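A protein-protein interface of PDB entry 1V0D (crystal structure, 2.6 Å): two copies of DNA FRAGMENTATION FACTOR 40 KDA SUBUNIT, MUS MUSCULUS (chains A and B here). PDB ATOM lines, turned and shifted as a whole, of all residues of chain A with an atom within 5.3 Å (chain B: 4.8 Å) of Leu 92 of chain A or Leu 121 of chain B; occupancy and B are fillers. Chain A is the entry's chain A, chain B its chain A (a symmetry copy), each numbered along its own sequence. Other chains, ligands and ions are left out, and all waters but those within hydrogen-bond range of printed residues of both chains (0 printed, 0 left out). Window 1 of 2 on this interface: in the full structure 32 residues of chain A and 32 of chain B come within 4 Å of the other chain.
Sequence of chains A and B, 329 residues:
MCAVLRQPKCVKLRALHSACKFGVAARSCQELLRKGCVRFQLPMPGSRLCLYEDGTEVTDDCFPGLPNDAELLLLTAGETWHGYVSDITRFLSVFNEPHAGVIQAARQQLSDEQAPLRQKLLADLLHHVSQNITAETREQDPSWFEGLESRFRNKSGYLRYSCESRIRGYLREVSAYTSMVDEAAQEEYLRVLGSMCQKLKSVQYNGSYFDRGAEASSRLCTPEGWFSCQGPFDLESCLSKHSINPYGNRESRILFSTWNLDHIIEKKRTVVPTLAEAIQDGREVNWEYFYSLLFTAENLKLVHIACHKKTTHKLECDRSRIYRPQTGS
Of the 10 printed residues of chain B, 6 touch a printed residue of chain A. Printed residues of chain B that touch a printed residue of chain A: Gln 109, Leu 117, Arg 118, Leu 121, Leu 122 and Leu 125. Hydrophobic or aromatic side chains of chain B that line the printed part of chain A: Leu 117, Leu 121, Leu 122 and Leu 125. Among the printed residues, 12 pairs touch across the chains. Among the printed residues, no Asp or Glu carboxylate lies within 4 Å of a Lys or Arg side-chain nitrogen of the other chain.
Position printed for both chains: 125. Of the 12 pairs that touch across the chains among the printed residues, none has its exchanged pair printed and touching as well.
Among the printed residues, merely in contact across the chains: His 128 of chain A with Leu 121 of chain B (3.1 Å), Asn 96 of chain A with Leu 117 of chain B (3.2 Å), Ile 88 of chain A with Gln 109 of chain B (3.2 Å), Leu 92 of chain A with Leu 122 of chain B (3.2 Å), Ile 88 of chain A with Leu 122 of chain B (3.3 Å), His 128 of chain A with Leu 117 of chain B (3.5 Å), Leu 92 of chain A with Gln 109 of chain B (3.6 Å), Phe 95 of chain A with Leu 121 of chain B (3.8 Å), Leu 92 of chain A with Leu 121 of chain B (3.8 Å) and Leu 92 of chain A with Leu 125 of chain B (3.8 Å).
The side-chain amide nitrogen of Gln 109 of chain B sits at hydrogen-bond distance from the side-chain hydroxyl of Thr 89 of chain A, at 3.4 Å. The backbone NH (N) of Arg 118 of chain B sits close to the side-chain amide nitrogen (ND2) of Asn 96 of chain A (3.4 Å).
Leu 92 of chain A touches just these residues of chain B: Gln 109, Leu 121, Leu 122 and Leu 125. Of the printed residues of chain B, Phe 95 of chain A touches Leu 121. Leu 125 of chain A touches none of the printed residues of chain B. Of the printed residues of chain B, His 128 of chain A touches Leu 117 and Leu 121. Printed residues of chain A within 4 Å of Arg 118 of chain B: Asn 96 (3.2 Å). Printed residues of chain A within 4 Å of Leu 121 of chain B: Leu 92 (3.8 Å), Phe 95 (3.8 Å) and His 128 (3.1 Å). Of the printed residues of chain A, Leu 122 of chain B touches Ile 88 and Leu 92. Ala 123 of chain B touches none of the printed residues of chain A. Printed residues of chain A within 4 Å of Leu 125 of chain B: Leu 92. The nearest residue of chain B that does not touch Leu 92 of chain A is Arg 118 of chain B (4.7 Å).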
ATOM      1  N   ILE A  88     -22.395  22.968  13.667  1.00  0.00           N
ATOM      2  CA  ILE A  88     -21.798  23.433  14.915  1.00  0.00           C
ATOM      3  C   ILE A  88     -20.687  22.578  15.529  1.00  0.00           C
ATOM      4  O   ILE A  88     -19.654  23.109  15.937  1.00  0.00           O
ATOM      5  CB  ILE A  88     -22.908  23.661  15.969  1.00  0.00           C
ATOM      6  CG1 ILE A  88     -22.293  23.918  17.344  1.00  0.00           C
ATOM      7  CG2 ILE A  88     -23.851  22.473  15.986  1.00  0.00           C
ATOM      8  CD1 ILE A  88     -23.318  24.224  18.409  1.00  0.00           C
ATOM      9  N   THR A  89     -20.894  21.267  15.606  1.00  0.00           N
ATOM     10  CA  THR A  89     -19.895  20.372  16.185  1.00  0.00           C
ATOM     11  C   THR A  89     -18.495  20.681  15.665  1.00  0.00           C
ATOM     12  O   THR A  89     -17.522  20.654  16.419  1.00  0.00           O
ATOM     13  CB  THR A  89     -20.215  18.902  15.871  1.00  0.00           C
ATOM     14  OG1 THR A  89     -21.527  18.589  16.351  1.00  0.00           O
ATOM     15  CG2 THR A  89     -19.208  17.983  16.542  1.00  0.00           C
ATOM     16  N   ARG A  90     -18.402  20.969  14.372  1.00  0.00           N
ATOM     17  CA  ARG A  90     -17.125  21.284  13.748  1.00  0.00           C
ATOM     18  C   ARG A  90     -16.623  22.635  14.249  1.00  0.00           C
ATOM     19  O   ARG A  90     -15.417  22.877  14.335  1.00  0.00           O
ATOM     20  CB  ARG A  90     -17.282  21.312  12.229  1.00  0.00           C
ATOM     21  N   PHE A  91     -17.565  23.506  14.589  1.00  0.00           N
ATOM     22  CA  PHE A  91     -17.253  24.844  15.072  1.00  0.00           C
ATOM     23  C   PHE A  91     -16.737  24.822  16.507  1.00  0.00           C
ATOM     24  O   PHE A  91     -15.643  25.315  16.783  1.00  0.00           O
ATOM     25  CB  PHE A  91     -18.500  25.725  14.950  1.00  0.00           C
ATOM     26  CG  PHE A  91     -19.014  25.845  13.536  1.00  0.00           C
ATOM     27  CD1 PHE A  91     -19.346  24.707  12.800  1.00  0.00           C
ATOM     28  CD2 PHE A  91     -19.141  27.093  12.931  1.00  0.00           C
ATOM     29  CE1 PHE A  91     -19.791  24.808  11.483  1.00  0.00           C
ATOM     30  CE2 PHE A  91     -19.587  27.206  11.611  1.00  0.00           C
ATOM     31  CZ  PHE A  91     -19.912  26.060  10.887  1.00  0.00           C
ATOM     32  N   LEU A  92     -17.519  24.247  17.418  1.00  0.00           N
ATOM     33  CA  LEU A  92     -17.111  24.153  18.818  1.00  0.00           C
ATOM     34  C   LEU A  92     -15.825  23.340  18.873  1.00  0.00           C
ATOM     35  O   LEU A  92     -15.084  23.384  19.853  1.00  0.00           O
ATOM     36  CB  LEU A  92     -18.180  23.433  19.645  1.00  0.00           C
ATOM     37  CG  LEU A  92     -19.595  24.005  19.743  1.00  0.00           C
ATOM     38  CD1 LEU A  92     -20.485  22.990  20.436  1.00  0.00           C
ATOM     39  CD2 LEU A  92     -19.587  25.321  20.507  1.00  0.00           C
ATOM     40  N   SER A  93     -15.578  22.597  17.800  1.00  0.00           N
ATOM     41  CA  SER A  93     -14.407  21.739  17.676  1.00  0.00           C
ATOM     42  C   SER A  93     -13.082  22.497  17.605  1.00  0.00           C
ATOM     43  O   SER A  93     -12.098  22.102  18.235  1.00  0.00           O
ATOM     44  CB  SER A  93     -14.558  20.853  16.436  1.00  0.00           C
ATOM     45  OG  SER A  93     -13.418  20.036  16.243  1.00  0.00           O
ATOM     46  N   VAL A  94     -13.061  23.583  16.842  1.00  0.00           N
ATOM     47  CA  VAL A  94     -11.849  24.378  16.676  1.00  0.00           C
ATOM     48  C   VAL A  94     -11.734  25.528  17.673  1.00  0.00           C
ATOM     49  O   VAL A  94     -10.634  25.882  18.103  1.00  0.00           O
ATOM     50  CB  VAL A  94     -11.780  24.968  15.257  1.00  0.00           C
ATOM     51  CG1 VAL A  94     -10.427  25.622  15.031  1.00  0.00           C
ATOM     52  CG2 VAL A  94     -12.041  23.877  14.229  1.00  0.00           C
ATOM     53  N   PHE A  95     -12.878  26.102  18.036  1.00  0.00           N
ATOM     54  CA  PHE A  95     -12.934  27.231  18.962  1.00  0.00           C
ATOM     55  C   PHE A  95     -12.743  26.910  20.436  1.00  0.00           C
ATOM     56  O   PHE A  95     -12.765  27.817  21.269  1.00  0.00           O
ATOM     57  CB  PHE A  95     -14.264  27.970  18.802  1.00  0.00           C
ATOM     58  CG  PHE A  95     -14.285  28.951  17.671  1.00  0.00           C
ATOM     59  CD1 PHE A  95     -15.301  28.914  16.721  1.00  0.00           C
ATOM     60  CD2 PHE A  95     -13.304  29.932  17.569  1.00  0.00           C
ATOM     61  CE1 PHE A  95     -15.344  29.842  15.683  1.00  0.00           C
ATOM     62  CE2 PHE A  95     -13.336  30.864  16.537  1.00  0.00           C
ATOM     63  CZ  PHE A  95     -14.360  30.819  15.591  1.00  0.00           C
ATOM     64  N   ASN A  96     -12.557  25.641  20.777  1.00  0.00           N
ATOM     65  CA  ASN A  96     -12.394  25.304  22.182  1.00  0.00           C
ATOM     66  C   ASN A  96     -10.946  25.167  22.632  1.00  0.00           C
ATOM     67  O   ASN A  96     -10.527  25.838  23.576  1.00  0.00           O
ATOM     68  CB  ASN A  96     -13.164  24.029  22.519  1.00  0.00           C
ATOM     69  CG  ASN A  96     -14.008  24.182  23.770  1.00  0.00           C
ATOM     70  OD1 ASN A  96     -13.498  24.511  24.840  1.00  0.00           O
ATOM     71  ND2 ASN A  96     -15.307  23.953  23.639  1.00  0.00           N
ATOM     72  N   LEU A 125     -15.366  35.279  21.866  1.00  0.00           N
ATOM     73  CA  LEU A 125     -14.579  34.117  21.480  1.00  0.00           C
ATOM     74  C   LEU A 125     -13.137  34.253  21.923  1.00  0.00           C
ATOM     75  O   LEU A 125     -12.561  33.324  22.478  1.00  0.00           O
ATOM     76  CB  LEU A 125     -14.641  33.909  19.971  1.00  0.00           C
ATOM     77  CG  LEU A 125     -15.906  33.164  19.546  1.00  0.00           C
ATOM     78  CD1 LEU A 125     -16.027  33.130  18.028  1.00  0.00           C
ATOM     79  CD2 LEU A 125     -15.853  31.750  20.124  1.00  0.00           C
ATOM     80  N   HIS A 128     -13.099  33.560  25.509  1.00  0.00           N
ATOM     81  CA  HIS A 128     -13.266  32.131  25.724  1.00  0.00           C
ATOM     82  C   HIS A 128     -11.991  31.337  25.497  1.00  0.00           C
ATOM     83  O   HIS A 128     -11.701  30.395  26.234  1.00  0.00           O
ATOM     84  CB  HIS A 128     -14.364  31.605  24.809  1.00  0.00           C
ATOM     85  CG  HIS A 128     -14.709  30.171  25.042  1.00  0.00           C
ATOM     86  ND1 HIS A 128     -13.832  29.142  24.776  1.00  0.00           N
ATOM     87  CD2 HIS A 128     -15.839  29.591  25.512  1.00  0.00           C
ATOM     88  CE1 HIS A 128     -14.407  27.989  25.071  1.00  0.00           C
ATOM     89  NE2 HIS A 128     -15.626  28.234  25.520  1.00  0.00           N
ATOM     90  N   GLN B 109     -27.676  20.120  22.078  1.00  0.00           N
ATOM     91  CA  GLN B 109     -26.340  19.741  22.512  1.00  0.00           C
ATOM     92  C   GLN B 109     -26.114  20.114  23.972  1.00  0.00           C
ATOM     93  O   GLN B 109     -25.275  19.519  24.645  1.00  0.00           O
ATOM     94  CB  GLN B 109     -25.281  20.396  21.638  1.00  0.00           C
ATOM     95  CG  GLN B 109     -25.185  19.792  20.262  1.00  0.00           C
ATOM     96  CD  GLN B 109     -23.831  20.037  19.632  1.00  0.00           C
ATOM     97  OE1 GLN B 109     -23.438  21.180  19.406  1.00  0.00           O
ATOM     98  NE2 GLN B 109     -23.102  18.961  19.354  1.00  0.00           N
ATOM     99  N   LEU B 117     -16.011  23.147  29.364  1.00  0.00           N
ATOM    100  CA  LEU B 117     -15.661  24.197  28.406  1.00  0.00           C
ATOM    101  C   LEU B 117     -16.610  24.247  27.217  1.00  0.00           C
ATOM    102  O   LEU B 117     -17.106  25.312  26.865  1.00  0.00           O
ATOM    103  CB  LEU B 117     -14.240  23.997  27.891  1.00  0.00           C
ATOM    104  CG  LEU B 117     -13.115  24.736  28.613  1.00  0.00           C
ATOM    105  CD1 LEU B 117     -11.775  24.179  28.165  1.00  0.00           C
ATOM    106  CD2 LEU B 117     -13.204  26.230  28.317  1.00  0.00           C
ATOM    107  N   ARG B 118     -16.851  23.094  26.595  1.00  0.00           N
ATOM    108  CA  ARG B 118     -17.746  23.017  25.441  1.00  0.00           C
ATOM    109  C   ARG B 118     -19.140  23.469  25.848  1.00  0.00           C
ATOM    110  O   ARG B 118     -19.841  24.127  25.083  1.00  0.00           O
ATOM    111  CB  ARG B 118     -17.793  21.580  24.889  1.00  0.00           C
ATOM    112  N   GLN B 119     -19.534  23.108  27.062  1.00  0.00           N
ATOM    113  CA  GLN B 119     -20.845  23.471  27.578  1.00  0.00           C
ATOM    114  C   GLN B 119     -20.921  24.987  27.703  1.00  0.00           C
ATOM    115  O   GLN B 119     -21.946  25.597  27.400  1.00  0.00           O
ATOM    116  CB  GLN B 119     -21.057  22.823  28.947  1.00  0.00           C
ATOM    117  CG  GLN B 119     -22.378  23.163  29.618  1.00  0.00           C
ATOM    118  CD  GLN B 119     -22.416  22.716  31.078  1.00  0.00           C
ATOM    119  OE1 GLN B 119     -22.213  21.533  31.391  1.00  0.00           O
ATOM    120  NE2 GLN B 119     -22.678  23.665  31.979  1.00  0.00           N
ATOM    121  N   LYS B 120     -19.818  25.580  28.152  1.00  0.00           N
ATOM    122  CA  LYS B 120     -19.703  27.027  28.339  1.00  0.00           C
ATOM    123  C   LYS B 120     -19.982  27.720  27.018  1.00  0.00           C
ATOM    124  O   LYS B 120     -21.006  28.381  26.851  1.00  0.00           O
ATOM    125  CB  LYS B 120     -18.289  27.371  28.804  1.00  0.00           C
ATOM    126  CG  LYS B 120     -18.222  28.372  29.916  1.00  0.00           C
ATOM    127  CD  LYS B 120     -18.804  29.689  29.495  1.00  0.00           C
ATOM    128  CE  LYS B 120     -18.719  30.700  30.623  1.00  0.00           C
ATOM    129  NZ  LYS B 120     -19.315  31.996  30.223  1.00  0.00           N
ATOM    130  N   LEU B 121     -19.056  27.542  26.083  1.00  0.00           N
ATOM    131  CA  LEU B 121     -19.150  28.118  24.750  1.00  0.00           C
ATOM    132  C   LEU B 121     -20.549  27.951  24.169  1.00  0.00           C
ATOM    133  O   LEU B 121     -21.119  28.875  23.582  1.00  0.00           O
ATOM    134  CB  LEU B 121     -18.134  27.438  23.836  1.00  0.00           C
ATOM    135  CG  LEU B 121     -17.499  28.281  22.731  1.00  0.00           C
ATOM    136  CD1 LEU B 121     -16.449  27.445  22.037  1.00  0.00           C
ATOM    137  CD2 LEU B 121     -18.552  28.761  21.746  1.00  0.00           C
ATOM    138  N   LEU B 122     -21.101  26.759  24.346  1.00  0.00           N
ATOM    139  CA  LEU B 122     -22.424  26.439  23.839  1.00  0.00           C
ATOM    140  C   LEU B 122     -23.492  27.272  24.534  1.00  0.00           C
ATOM    141  O   LEU B 122     -24.409  27.789  23.892  1.00  0.00           O
ATOM    142  CB  LEU B 122     -22.705  24.952  24.050  1.00  0.00           C
ATOM    143  CG  LEU B 122     -23.634  24.305  23.024  1.00  0.00           C
ATOM    144  CD1 LEU B 122     -23.051  24.528  21.636  1.00  0.00           C
ATOM    145  CD2 LEU B 122     -23.782  22.819  23.311  1.00  0.00           C
ATOM    146  N   ALA B 123     -23.381  27.398  25.852  1.00  0.00           N
ATOM    147  CA  ALA B 123     -24.349  28.177  26.612  1.00  0.00           C
ATOM    148  C   ALA B 123     -24.241  29.628  26.169  1.00  0.00           C
ATOM    149  O   ALA B 123     -25.250  30.309  25.970  1.00  0.00           O
ATOM    150  CB  ALA B 123     -24.069  28.060  28.096  1.00  0.00           C
ATOM    151  N   ASP B 124     -23.004  30.090  26.008  1.00  0.00           N
ATOM    152  CA  ASP B 124     -22.754  31.453  25.583  1.00  0.00           C
ATOM    153  C   ASP B 124     -23.334  31.709  24.202  1.00  0.00           C
ATOM    154  O   ASP B 124     -24.025  32.708  23.988  1.00  0.00           O
ATOM    155  CB  ASP B 124     -21.257  31.741  25.579  1.00  0.00           C
ATOM    156  CG  ASP B 124     -20.671  31.803  26.982  1.00  0.00           C
ATOM    157  OD1 ASP B 124     -21.354  32.324  27.897  1.00  0.00           O
ATOM    158  OD2 ASP B 124     -19.520  31.346  27.167  1.00  0.00           O
ATOM    159  N   LEU B 125     -23.059  30.804  23.267  1.00  0.00           N
ATOM    160  CA  LEU B 125     -23.571  30.947  21.911  1.00  0.00           C
ATOM    161  C   LEU B 125     -25.081  31.062  21.898  1.00  0.00           C
ATOM    162  O   LEU B 125     -25.638  31.921  21.225  1.00  0.00           O
ATOM    163  CB  LEU B 125     -23.132  29.767  21.050  1.00  0.00           C
ATOM    164  CG  LEU B 125     -21.714  29.946  20.509  1.00  0.00           C
ATOM    165  CD1 LEU B 125     -21.242  28.679  19.807  1.00  0.00           C
ATOM    166  CD2 LEU B 125     -21.708  31.139  19.553  1.00  0.00           C
